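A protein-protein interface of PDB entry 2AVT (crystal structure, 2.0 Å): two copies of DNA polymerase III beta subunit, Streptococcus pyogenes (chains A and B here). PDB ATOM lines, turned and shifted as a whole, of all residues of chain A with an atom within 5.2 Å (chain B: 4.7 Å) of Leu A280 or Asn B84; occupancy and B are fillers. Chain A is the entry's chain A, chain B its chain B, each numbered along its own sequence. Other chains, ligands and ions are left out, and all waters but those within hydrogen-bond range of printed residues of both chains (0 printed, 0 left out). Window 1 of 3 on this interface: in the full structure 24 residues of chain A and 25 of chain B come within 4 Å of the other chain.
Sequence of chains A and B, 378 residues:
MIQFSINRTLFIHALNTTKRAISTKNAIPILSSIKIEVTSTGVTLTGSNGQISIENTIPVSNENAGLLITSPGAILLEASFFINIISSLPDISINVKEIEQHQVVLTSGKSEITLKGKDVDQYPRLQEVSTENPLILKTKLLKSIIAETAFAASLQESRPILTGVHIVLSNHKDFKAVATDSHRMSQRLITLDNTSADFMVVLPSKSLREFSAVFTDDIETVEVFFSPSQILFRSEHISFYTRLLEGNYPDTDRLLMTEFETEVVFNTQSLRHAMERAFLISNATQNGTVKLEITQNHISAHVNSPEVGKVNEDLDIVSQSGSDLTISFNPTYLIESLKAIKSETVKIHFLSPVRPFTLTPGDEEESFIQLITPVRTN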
ATOM      1  N   GLU A 276      25.009 -24.804 -14.476  1.00  0.00           N
ATOM      2  CA  GLU A 276      23.969 -23.805 -14.705  1.00  0.00           C
ATOM      3  C   GLU A 276      23.638 -23.113 -13.378  1.00  0.00           C
ATOM      4  O   GLU A 276      23.387 -21.910 -13.347  1.00  0.00           O
ATOM      5  CB  GLU A 276      22.726 -24.458 -15.330  1.00  0.00           C
ATOM      6  CG  GLU A 276      22.983 -24.969 -16.753  1.00  0.00           C
ATOM      7  CD  GLU A 276      21.810 -25.724 -17.360  1.00  0.00           C
ATOM      8  OE1 GLU A 276      21.098 -26.425 -16.616  1.00  0.00           O
ATOM      9  OE2 GLU A 276      21.616 -25.633 -18.591  1.00  0.00           O
ATOM     10  N   ARG A 277      23.662 -23.870 -12.282  1.00  0.00           N
ATOM     11  CA  ARG A 277      23.393 -23.303 -10.966  1.00  0.00           C
ATOM     12  C   ARG A 277      24.552 -22.399 -10.574  1.00  0.00           C
ATOM     13  O   ARG A 277      24.359 -21.349  -9.958  1.00  0.00           O
ATOM     14  CB  ARG A 277      23.266 -24.393  -9.911  1.00  0.00           C
ATOM     15  CG  ARG A 277      22.140 -25.358 -10.121  1.00  0.00           C
ATOM     16  CD  ARG A 277      22.077 -26.316  -8.952  1.00  0.00           C
ATOM     17  NE  ARG A 277      21.274 -27.485  -9.278  1.00  0.00           N
ATOM     18  CZ  ARG A 277      21.684 -28.473 -10.063  1.00  0.00           C
ATOM     19  NH1 ARG A 277      22.896 -28.443 -10.593  1.00  0.00           N
ATOM     20  NH2 ARG A 277      20.867 -29.476 -10.344  1.00  0.00           N
ATOM     21  N   ALA A 278      25.760 -22.824 -10.922  1.00  0.00           N
ATOM     22  CA  ALA A 278      26.952 -22.056 -10.609  1.00  0.00           C
ATOM     23  C   ALA A 278      26.876 -20.706 -11.302  1.00  0.00           C
ATOM     24  O   ALA A 278      27.310 -19.692 -10.757  1.00  0.00           O
ATOM     25  CB  ALA A 278      28.197 -22.811 -11.066  1.00  0.00           C
ATOM     26  N   PHE A 279      26.315 -20.700 -12.508  1.00  0.00           N
ATOM     27  CA  PHE A 279      26.184 -19.475 -13.282  1.00  0.00           C
ATOM     28  C   PHE A 279      25.191 -18.505 -12.644  1.00  0.00           C
ATOM     29  O   PHE A 279      25.404 -17.295 -12.659  1.00  0.00           O
ATOM     30  CB  PHE A 279      25.740 -19.793 -14.712  1.00  0.00           C
ATOM     31  CG  PHE A 279      25.619 -18.581 -15.591  1.00  0.00           C
ATOM     32  CD1 PHE A 279      26.718 -17.769 -15.826  1.00  0.00           C
ATOM     33  CD2 PHE A 279      24.408 -18.248 -16.172  1.00  0.00           C
ATOM     34  CE1 PHE A 279      26.610 -16.645 -16.626  1.00  0.00           C
ATOM     35  CE2 PHE A 279      24.291 -17.128 -16.974  1.00  0.00           C
ATOM     36  CZ  PHE A 279      25.393 -16.323 -17.203  1.00  0.00           C
ATOM     37  N   LEU A 280      24.110 -19.036 -12.080  1.00  0.00           N
ATOM     38  CA  LEU A 280      23.100 -18.192 -11.447  1.00  0.00           C
ATOM     39  C   LEU A 280      23.656 -17.333 -10.315  1.00  0.00           C
ATOM     40  O   LEU A 280      23.027 -16.354  -9.906  1.00  0.00           O
ATOM     41  CB  LEU A 280      21.940 -19.044 -10.919  1.00  0.00           C
ATOM     42  CG  LEU A 280      21.023 -19.632 -11.995  1.00  0.00           C
ATOM     43  CD1 LEU A 280      19.940 -20.481 -11.349  1.00  0.00           C
ATOM     44  CD2 LEU A 280      20.409 -18.503 -12.816  1.00  0.00           C
ATOM     45  N   ILE A 281      24.834 -17.689  -9.811  1.00  0.00           N
ATOM     46  CA  ILE A 281      25.438 -16.923  -8.728  1.00  0.00           C
ATOM     47  C   ILE A 281      26.658 -16.150  -9.208  1.00  0.00           C
ATOM     48  O   ILE A 281      26.844 -14.981  -8.858  1.00  0.00           O
ATOM     49  CB  ILE A 281      25.853 -17.842  -7.563  1.00  0.00           C
ATOM     50  CG1 ILE A 281      24.639 -18.627  -7.068  1.00  0.00           C
ATOM     51  CG2 ILE A 281      26.458 -17.017  -6.438  1.00  0.00           C
ATOM     52  CD1 ILE A 281      23.458 -17.768  -6.691  1.00  0.00           C
ATOM     53  N   SER A 282      27.483 -16.800 -10.020  1.00  0.00           N
ATOM     54  CA  SER A 282      28.688 -16.169 -10.538  1.00  0.00           C
ATOM     55  C   SER A 282      28.327 -15.033 -11.487  1.00  0.00           C
ATOM     56  O   SER A 282      29.100 -14.087 -11.665  1.00  0.00           O
ATOM     57  CB  SER A 282      29.547 -17.197 -11.285  1.00  0.00           C
ATOM     58  OG  SER A 282      28.970 -17.545 -12.534  1.00  0.00           O
ATOM     59  N   ASN A 283      27.151 -15.131 -12.096  1.00  0.00           N
ATOM     60  CA  ASN A 283      26.702 -14.116 -13.039  1.00  0.00           C
ATOM     61  C   ASN A 283      26.416 -12.794 -12.326  1.00  0.00           C
ATOM     62  O   ASN A 283      26.449 -11.726 -12.942  1.00  0.00           O
ATOM     63  CB  ASN A 283      25.452 -14.603 -13.782  1.00  0.00           C
ATOM     64  CG  ASN A 283      25.129 -13.756 -14.994  1.00  0.00           C
ATOM     65  OD1 ASN A 283      25.985 -13.521 -15.846  1.00  0.00           O
ATOM     66  ND2 ASN A 283      23.889 -13.298 -15.080  1.00  0.00           N
ATOM     67  N   ALA A 284      26.145 -12.875 -11.025  1.00  0.00           N
ATOM     68  CA  ALA A 284      25.865 -11.686 -10.231  1.00  0.00           C
ATOM     69  C   ALA A 284      27.073 -10.766 -10.280  1.00  0.00           C
ATOM     70  O   ALA A 284      26.942  -9.556 -10.466  1.00  0.00           O
ATOM     71  CB  ALA A 284      25.557 -12.074  -8.789  1.00  0.00           C
ATOM     72  N   SER B  80      12.876 -12.767  -8.829  1.00  0.00           N
ATOM     73  CA  SER B  80      13.419 -13.450 -10.005  1.00  0.00           C
ATOM     74  C   SER B  80      14.615 -14.333  -9.674  1.00  0.00           C
ATOM     75  O   SER B  80      14.634 -15.521 -10.001  1.00  0.00           O
ATOM     76  CB  SER B  80      13.827 -12.431 -11.070  1.00  0.00           C
ATOM     77  OG  SER B  80      12.699 -11.729 -11.556  1.00  0.00           O
ATOM     78  N   PHE B  81      15.607 -13.738  -9.019  1.00  0.00           N
ATOM     79  CA  PHE B  81      16.822 -14.438  -8.628  1.00  0.00           C
ATOM     80  C   PHE B  81      16.522 -15.725  -7.860  1.00  0.00           C
ATOM     81  O   PHE B  81      17.021 -16.796  -8.210  1.00  0.00           O
ATOM     82  CB  PHE B  81      17.686 -13.512  -7.770  1.00  0.00           C
ATOM     83  CG  PHE B  81      18.983 -14.124  -7.337  1.00  0.00           C
ATOM     84  CD1 PHE B  81      19.910 -14.549  -8.274  1.00  0.00           C
ATOM     85  CD2 PHE B  81      19.283 -14.257  -5.992  1.00  0.00           C
ATOM     86  CE1 PHE B  81      21.111 -15.098  -7.877  1.00  0.00           C
ATOM     87  CE2 PHE B  81      20.483 -14.804  -5.586  1.00  0.00           C
ATOM     88  CZ  PHE B  81      21.401 -15.225  -6.531  1.00  0.00           C
ATOM     89  N   PHE B  82      15.705 -15.610  -6.818  1.00  0.00           N
ATOM     90  CA  PHE B  82      15.328 -16.752  -5.989  1.00  0.00           C
ATOM     91  C   PHE B  82      14.532 -17.785  -6.775  1.00  0.00           C
ATOM     92  O   PHE B  82      14.733 -18.993  -6.628  1.00  0.00           O
ATOM     93  CB  PHE B  82      14.490 -16.280  -4.800  1.00  0.00           C
ATOM     94  CG  PHE B  82      13.983 -17.394  -3.929  1.00  0.00           C
ATOM     95  CD1 PHE B  82      14.852 -18.120  -3.128  1.00  0.00           C
ATOM     96  CD2 PHE B  82      12.634 -17.709  -3.899  1.00  0.00           C
ATOM     97  CE1 PHE B  82      14.382 -19.134  -2.316  1.00  0.00           C
ATOM     98  CE2 PHE B  82      12.162 -18.722  -3.088  1.00  0.00           C
ATOM     99  CZ  PHE B  82      13.038 -19.435  -2.295  1.00  0.00           C
ATOM    100  N   ILE B  83      13.612 -17.307  -7.602  1.00  0.00           N
ATOM    101  CA  ILE B  83      12.794 -18.208  -8.391  1.00  0.00           C
ATOM    102  C   ILE B  83      13.671 -18.983  -9.363  1.00  0.00           C
ATOM    103  O   ILE B  83      13.490 -20.184  -9.531  1.00  0.00           O
ATOM    104  CB  ILE B  83      11.695 -17.437  -9.151  1.00  0.00           C
ATOM    105  CG1 ILE B  83      10.810 -16.697  -8.143  1.00  0.00           C
ATOM    106  CG2 ILE B  83      10.862 -18.399  -9.980  1.00  0.00           C
ATOM    107  CD1 ILE B  83       9.648 -15.934  -8.766  1.00  0.00           C
ATOM    108  N   ASN B  84      14.627 -18.309  -9.995  1.00  0.00           N
ATOM    109  CA  ASN B  84      15.525 -18.998 -10.915  1.00  0.00           C
ATOM    110  C   ASN B  84      16.246 -20.105 -10.141  1.00  0.00           C
ATOM    111  O   ASN B  84      16.247 -21.266 -10.547  1.00  0.00           O
ATOM    112  CB  ASN B  84      16.570 -18.038 -11.496  1.00  0.00           C
ATOM    113  CG  ASN B  84      15.966 -16.998 -12.404  1.00  0.00           C
ATOM    114  OD1 ASN B  84      15.108 -17.303 -13.230  1.00  0.00           O
ATOM    115  ND2 ASN B  84      16.422 -15.757 -12.269  1.00  0.00           N
ATOM    116  N   ILE B  85      16.851 -19.728  -9.018  1.00  0.00           N
ATOM    117  CA  ILE B  85      17.578 -20.676  -8.183  1.00  0.00           C
ATOM    118  C   ILE B  85      16.770 -21.922  -7.859  1.00  0.00           C
ATOM    119  O   ILE B  85      17.229 -23.037  -8.090  1.00  0.00           O
ATOM    120  CB  ILE B  85      18.021 -20.034  -6.850  1.00  0.00           C
ATOM    121  CG1 ILE B  85      19.078 -18.961  -7.111  1.00  0.00           C
ATOM    122  CG2 ILE B  85      18.561 -21.108  -5.913  1.00  0.00           C
ATOM    123  CD1 ILE B  85      20.300 -19.478  -7.840  1.00  0.00           C
ATOM    124  N   ILE B  86      15.570 -21.740  -7.321  1.00  0.00           N
ATOM    125  CA  ILE B  86      14.725 -22.873  -6.962  1.00  0.00           C
ATOM    126  C   ILE B  86      14.465 -23.790  -8.154  1.00  0.00           C
ATOM    127  O   ILE B  86      14.526 -25.018  -8.034  1.00  0.00           O
ATOM    128  CB  ILE B  86      13.371 -22.399  -6.379  1.00  0.00           C
ATOM    129  CG1 ILE B  86      13.602 -21.706  -5.033  1.00  0.00           C
ATOM    130  CG2 ILE B  86      12.437 -23.582  -6.170  1.00  0.00           C
ATOM    131  CD1 ILE B  86      14.129 -22.643  -3.960  1.00  0.00           C
ATOM    132  N   SER B  87      14.188 -23.195  -9.311  1.00  0.00           N
ATOM    133  CA  SER B  87      13.917 -23.973 -10.512  1.00  0.00           C
ATOM    134  C   SER B  87      15.099 -24.846 -10.930  1.00  0.00           C
ATOM    135  O   SER B  87      14.911 -25.927 -11.481  1.00  0.00           O
ATOM    136  CB  SER B  87      13.538 -23.044 -11.667  1.00  0.00           C
ATOM    137  OG  SER B  87      12.309 -22.394 -11.415  1.00  0.00           O
ATOM    138  N   SER B  88      16.315 -24.380 -10.658  1.00  0.00           N
ATOM    139  CA  SER B  88      17.517 -25.119 -11.036  1.00  0.00           C
ATOM    140  C   SER B  88      17.989 -26.123  -9.994  1.00  0.00           C
ATOM    141  O   SER B  88      19.034 -26.737 -10.169  1.00  0.00           O
ATOM    142  CB  SER B  88      18.665 -24.154 -11.318  1.00  0.00           C
ATOM    143  OG  SER B  88      19.243 -23.708 -10.105  1.00  0.00           O
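No position is printed for both chains.
Of the 7 pairs that touch across the chains among the printed residues, none has its exchanged pair printed and touching as well.
O of Ser B88 lies within hydrogen-bond range of NE of Arg A277 (2.5 Å).
The backbone carbonyl oxygen (O) of Ser B80 sits at hydrogen-bond distance from the side-chain amide nitrogen (ND2) of Asn B84, at 2.9 Å.
The backbone carbonyl oxygen (O) of Ile B85 is in hydrogen-bond range of the side-chain hydroxyl (OG) of Ser B88, 2.9 Å away.
Printed residues of chain A that touch a printed residue of chain B: Arg A277, Leu A280 and Ile A281.
Hydrophobic or aromatic side chains of chain A within 4 Å of the printed part of chain B: Leu A280 and Ile A281.
Among the printed residues, no Asp or Glu carboxylate lies within 4 Å of a Lys or Arg side-chain nitrogen of the other chain.
Of chain B, only Phe B81 (3.1 Å), Asn B84 (3.9 Å), Ile B85 (3.5 Å) and Ser B88 (3.5 Å) come within 4 Å of Leu A280.
Asn B84 touches just one residue of chain A: Leu A280 (3.9 Å).
Printed residues of chain B within 4 Å of Arg A277: Ser B88 (2.5 Å).
Printed residues of chain B within 4 Å of Ile A281: Phe B81 and Ile B85.
Of the printed residues of chain A, Phe B81 touches Leu A280 (3.1 Å) and Ile A281 (3.3 Å).
Printed residues of chain A within 4 Å of Ile B85: Leu A280 and Ile A281.
Of the printed residues of chain A, Ser B88 touches Arg A277 and Leu A280.
Glu A276 touches none of the printed residues of chain B.
Ser B80 touches none of the printed residues of chain A.
The nearest printed residue of chain A that does not touch Asn B84 is Arg A277 (7.2 Å).
Among the printed residues, merely in contact across the chains: Leu A280 with Phe B81 (3.1 Å), Ile A281 with Phe B81 (3.3 Å), Leu A280 with Ile B85 (3.5 Å), Leu A280 with Ser B88 (3.5 Å), Ile A281 with Ile B85 (3.8 Å) and Leu A280 with Asn B84 (3.9 Å).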
